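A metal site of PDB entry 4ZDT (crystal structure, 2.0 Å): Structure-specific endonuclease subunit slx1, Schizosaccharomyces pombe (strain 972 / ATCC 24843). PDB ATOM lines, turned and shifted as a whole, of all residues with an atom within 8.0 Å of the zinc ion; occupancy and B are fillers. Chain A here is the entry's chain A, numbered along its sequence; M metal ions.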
ATOM      1  N   LYS A   5     -20.220   9.618  -7.201  1.00  0.00           N
ATOM      2  CA  LYS A   5     -21.258  10.146  -6.322  1.00  0.00           C
ATOM      3  C   LYS A   5     -21.577   9.147  -5.217  1.00  0.00           C
ATOM      4  O   LYS A   5     -21.783   7.961  -5.496  1.00  0.00           O
ATOM      5  CB  LYS A   5     -22.503  10.403  -7.150  1.00  0.00           C
ATOM      6  CG  LYS A   5     -23.582  11.240  -6.498  1.00  0.00           C
ATOM      7  CD  LYS A   5     -24.681  11.571  -7.508  1.00  0.00           C
ATOM      8  CE  LYS A   5     -25.458  12.813  -7.085  1.00  0.00           C
ATOM      9  NZ  LYS A   5     -26.689  13.022  -7.904  1.00  0.00           N
ATOM     10  N   CYS A   6     -21.640   9.614  -3.970  1.00  0.00           N
ATOM     11  CA  CYS A   6     -22.139   8.757  -2.906  1.00  0.00           C
ATOM     12  C   CYS A   6     -23.633   8.507  -3.100  1.00  0.00           C
ATOM     13  O   CYS A   6     -24.418   9.436  -3.312  1.00  0.00           O
ATOM     14  CB  CYS A   6     -21.874   9.361  -1.515  1.00  0.00           C
ATOM     15  SG  CYS A   6     -22.828   8.518  -0.210  1.00  0.00           S
ATOM     16  N   ASN A   7     -24.021   7.240  -2.990  1.00  0.00           N
ATOM     17  CA  ASN A   7     -25.412   6.846  -3.212  1.00  0.00           C
ATOM     18  C   ASN A   7     -26.348   7.042  -2.020  1.00  0.00           C
ATOM     19  O   ASN A   7     -27.484   6.570  -2.038  1.00  0.00           O
ATOM     20  CB  ASN A   7     -25.477   5.393  -3.690  1.00  0.00           C
ATOM     21  CG  ASN A   7     -25.171   4.405  -2.583  1.00  0.00           C
ATOM     22  OD1 ASN A   7     -24.578   4.755  -1.562  1.00  0.00           O
ATOM     23  ND2 ASN A   7     -25.585   3.155  -2.763  1.00  0.00           N
ATOM     24  N   LEU A   8     -25.881   7.741  -0.991  1.00  0.00           N
ATOM     25  CA  LEU A   8     -26.738   7.991   0.166  1.00  0.00           C
ATOM     26  C   LEU A   8     -26.888   9.483   0.483  1.00  0.00           C
ATOM     27  O   LEU A   8     -27.936   9.905   0.988  1.00  0.00           O
ATOM     28  CB  LEU A   8     -26.207   7.247   1.399  1.00  0.00           C
ATOM     29  CG  LEU A   8     -26.155   5.707   1.311  1.00  0.00           C
ATOM     30  CD1 LEU A   8     -25.373   5.086   2.481  1.00  0.00           C
ATOM     31  CD2 LEU A   8     -27.564   5.093   1.225  1.00  0.00           C
ATOM     32  N   CYS A   9     -25.837  10.276   0.196  1.00  0.00           N
ATOM     33  CA  CYS A   9     -25.846  11.713   0.491  1.00  0.00           C
ATOM     34  C   CYS A   9     -25.705  12.586  -0.774  1.00  0.00           C
ATOM     35  O   CYS A   9     -25.858  13.816  -0.702  1.00  0.00           O
ATOM     36  CB  CYS A   9     -24.750  12.063   1.484  1.00  0.00           C
ATOM     37  SG  CYS A   9     -23.135  12.317   0.741  1.00  0.00           S
ATOM     38  N   TYR A  10     -25.381  11.947  -1.901  1.00  0.00           N
ATOM     39  CA  TYR A  10     -25.337  12.575  -3.218  1.00  0.00           C
ATOM     40  C   TYR A  10     -24.221  13.602  -3.426  1.00  0.00           C
ATOM     41  O   TYR A  10     -24.175  14.256  -4.490  1.00  0.00           O
ATOM     42  CB  TYR A  10     -26.720  13.141  -3.625  1.00  0.00           C
ATOM     43  CG  TYR A  10     -27.848  12.181  -3.323  1.00  0.00           C
ATOM     44  CD1 TYR A  10     -27.950  10.959  -3.979  1.00  0.00           C
ATOM     45  CD2 TYR A  10     -28.796  12.495  -2.347  1.00  0.00           C
ATOM     46  CE1 TYR A  10     -28.963  10.069  -3.681  1.00  0.00           C
ATOM     47  CE2 TYR A  10     -29.830  11.612  -2.043  1.00  0.00           C
ATOM     48  CZ  TYR A  10     -29.903  10.396  -2.713  1.00  0.00           C
ATOM     49  OH  TYR A  10     -30.913   9.512  -2.427  1.00  0.00           O
ATOM     50  N   GLU A  11     -23.336  13.737  -2.441  1.00  0.00           N
ATOM     51  CA  GLU A  11     -22.128  14.544  -2.616  1.00  0.00           C
ATOM     52  C   GLU A  11     -21.085  13.733  -3.355  1.00  0.00           C
ATOM     53  O   GLU A  11     -21.126  12.493  -3.350  1.00  0.00           O
ATOM     54  CB  GLU A  11     -21.555  15.027  -1.267  1.00  0.00           C
ATOM     55  CG  GLU A  11     -22.562  15.705  -0.328  1.00  0.00           C
ATOM     56  CD  GLU A  11     -23.136  16.997  -0.888  1.00  0.00           C
ATOM     57  OE1 GLU A  11     -22.363  17.792  -1.470  1.00  0.00           O
ATOM     58  OE2 GLU A  11     -24.364  17.213  -0.740  1.00  0.00           O
ATOM     59  N   CYS A  12     -20.162  14.422  -4.007  1.00  0.00           N
ATOM     60  CA  CYS A  12     -19.111  13.769  -4.752  1.00  0.00           C
ATOM     61  C   CYS A  12     -18.090  13.129  -3.829  1.00  0.00           C
ATOM     62  O   CYS A  12     -17.849  13.627  -2.729  1.00  0.00           O
ATOM     63  CB  CYS A  12     -18.439  14.727  -5.744  1.00  0.00           C
ATOM     64  SG  CYS A  12     -19.338  15.113  -7.249  1.00  0.00           S
ATOM     65  N   ILE A  13     -17.528  12.009  -4.271  1.00  0.00           N
ATOM     66  CA  ILE A  13     -16.470  11.334  -3.549  1.00  0.00           C
ATOM     67  C   ILE A  13     -15.168  11.635  -4.265  1.00  0.00           C
ATOM     68  O   ILE A  13     -14.986  11.243  -5.412  1.00  0.00           O
ATOM     69  CB  ILE A  13     -16.703   9.792  -3.449  1.00  0.00           C
ATOM     70  CG1 ILE A  13     -18.069   9.497  -2.803  1.00  0.00           C
ATOM     71  CG2 ILE A  13     -15.583   9.122  -2.676  1.00  0.00           C
ATOM     72  CD1 ILE A  13     -18.463   8.013  -2.810  1.00  0.00           C
ATOM     73  N   GLU A  17     -10.259  10.003  -1.507  1.00  0.00           N
ATOM     74  CA  GLU A  17     -11.147   9.634  -0.421  1.00  0.00           C
ATOM     75  C   GLU A  17     -11.425   8.129  -0.422  1.00  0.00           C
ATOM     76  O   GLU A  17     -11.616   7.534  -1.476  1.00  0.00           O
ATOM     77  CB  GLU A  17     -12.459  10.413  -0.553  1.00  0.00           C
ATOM     78  CG  GLU A  17     -13.106  10.743   0.778  1.00  0.00           C
ATOM     79  CD  GLU A  17     -14.267  11.710   0.644  1.00  0.00           C
ATOM     80  OE1 GLU A  17     -14.898  12.029   1.677  1.00  0.00           O
ATOM     81  OE2 GLU A  17     -14.565  12.160  -0.492  1.00  0.00           O
ATOM     82  N   ILE A  30     -21.894   2.266  -4.374  1.00  0.00           N
ATOM     83  CA  ILE A  30     -20.766   3.046  -3.861  1.00  0.00           C
ATOM     84  C   ILE A  30     -21.265   4.160  -2.926  1.00  0.00           C
ATOM     85  O   ILE A  30     -22.273   4.827  -3.207  1.00  0.00           O
ATOM     86  CB  ILE A  30     -19.850   3.574  -4.994  1.00  0.00           C
ATOM     87  CG1 ILE A  30     -19.186   2.376  -5.729  1.00  0.00           C
ATOM     88  CG2 ILE A  30     -18.739   4.481  -4.452  1.00  0.00           C
ATOM     89  CD1 ILE A  30     -18.504   2.725  -7.059  1.00  0.00           C
ATOM     90  N   ASN A  31     -20.549   4.374  -1.823  1.00  0.00           N
ATOM     91  CA  ASN A  31     -20.929   5.411  -0.870  1.00  0.00           C
ATOM     92  C   ASN A  31     -19.835   5.727   0.142  1.00  0.00           C
ATOM     93  O   ASN A  31     -18.910   4.934   0.343  1.00  0.00           O
ATOM     94  CB  ASN A  31     -22.219   5.026  -0.143  1.00  0.00           C
ATOM     95  CG  ASN A  31     -22.302   3.543   0.154  1.00  0.00           C
ATOM     96  OD1 ASN A  31     -21.399   2.970   0.772  1.00  0.00           O
ATOM     97  ND2 ASN A  31     -23.385   2.909  -0.282  1.00  0.00           N
ATOM     98  N   HIS A  32     -19.944   6.894   0.789  1.00  0.00           N
ATOM     99  CA  HIS A  32     -18.966   7.313   1.802  1.00  0.00           C
ATOM    100  C   HIS A  32     -19.018   6.297   2.933  1.00  0.00           C
ATOM    101  O   HIS A  32     -20.086   5.807   3.264  1.00  0.00           O
ATOM    102  CB  HIS A  32     -19.350   8.670   2.425  1.00  0.00           C
ATOM    103  CG  HIS A  32     -19.127   9.842   1.542  1.00  0.00           C
ATOM    104  ND1 HIS A  32     -20.169  10.553   0.972  1.00  0.00           N
ATOM    105  CD2 HIS A  32     -17.989  10.459   1.140  1.00  0.00           C
ATOM    106  CE1 HIS A  32     -19.675  11.548   0.258  1.00  0.00           C
ATOM    107  NE2 HIS A  32     -18.355  11.517   0.350  1.00  0.00           N
ATOM    108  N   LEU A  33     -17.862   5.981   3.510  1.00  0.00           N
ATOM    109  CA  LEU A  33     -17.812   5.096   4.697  1.00  0.00           C
ATOM    110  C   LEU A  33     -18.728   5.582   5.782  1.00  0.00           C
ATOM    111  O   LEU A  33     -19.507   4.800   6.320  1.00  0.00           O
ATOM    112  CB  LEU A  33     -16.386   4.998   5.245  1.00  0.00           C
ATOM    113  CG  LEU A  33     -15.346   4.330   4.351  1.00  0.00           C
ATOM    114  CD1 LEU A  33     -13.946   4.542   4.912  1.00  0.00           C
ATOM    115  CD2 LEU A  33     -15.659   2.805   4.255  1.00  0.00           C
ATOM    116  N   THR A  34     -18.626   6.869   6.126  1.00  0.00           N
ATOM    117  CA  THR A  34     -19.446   7.405   7.217  1.00  0.00           C
ATOM    118  C   THR A  34     -20.925   7.353   6.886  1.00  0.00           C
ATOM    119  O   THR A  34     -21.730   6.989   7.745  1.00  0.00           O
ATOM    120  CB  THR A  34     -19.017   8.833   7.652  1.00  0.00           C
ATOM    121  OG1 THR A  34     -18.982   9.672   6.501  1.00  0.00           O
ATOM    122  CG2 THR A  34     -17.640   8.784   8.244  1.00  0.00           C
ATOM    123  N   CYS A  35     -21.294   7.680   5.651  1.00  0.00           N
ATOM    124  CA  CYS A  35     -22.699   7.575   5.240  1.00  0.00           C
ATOM    125  C   CYS A  35     -23.263   6.157   5.400  1.00  0.00           C
ATOM    126  O   CYS A  35     -24.316   5.953   5.987  1.00  0.00           O
ATOM    127  CB  CYS A  35     -22.905   8.049   3.786  1.00  0.00           C
ATOM    128  SG  CYS A  35     -22.603   9.810   3.603  1.00  0.00           S
ATOM    129  N   LEU A  36     -22.563   5.164   4.826  1.00  0.00           N
ATOM    130  CA  LEU A  36     -22.994   3.766   4.943  1.00  0.00           C
ATOM    131  C   LEU A  36     -23.042   3.326   6.419  1.00  0.00           C
ATOM    132  O   LEU A  36     -23.999   2.722   6.845  1.00  0.00           O
ATOM    133  CB  LEU A  36     -22.049   2.832   4.154  1.00  0.00           C
ATOM    134  CG  LEU A  36     -22.532   1.394   3.951  1.00  0.00           C
ATOM    135  CD1 LEU A  36     -23.844   1.343   3.188  1.00  0.00           C
ATOM    136  CD2 LEU A  36     -21.488   0.541   3.221  1.00  0.00           C
HETATM  137 ZN    ZN M   1     -22.144  10.201   1.406  1.00  0.00          ZN
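The side-chain sulfur of Cys 9 lies close to the backbone NH of Glu 11.
SG of Cys 6 lies close to N of Leu 8, at 3.2 Å.
The backbone carbonyl oxygen (O) of Glu 11 lies within hydrogen-bond range of the backbone NH (N) of Cys 6 (3.0 Å).
Of the 17 residues printed, 4 come within 4 Å of the zinc ion.
Along chain A the residues within 4 Å of the zinc ion span positions 6 to 35.
The nearest printed residue that does not touch the zinc ion is Leu 8 (4.9 Å).
ND1 of His 32 binds the zinc ion, 2.1 Å away.
The side-chain sulfur (SG) of Cys 35 binds the zinc ion.
SG of Cys 9 is bound to the zinc ion (2.4 Å).
The zinc ion is bound by SG of Cys 6 (2.4 Å).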
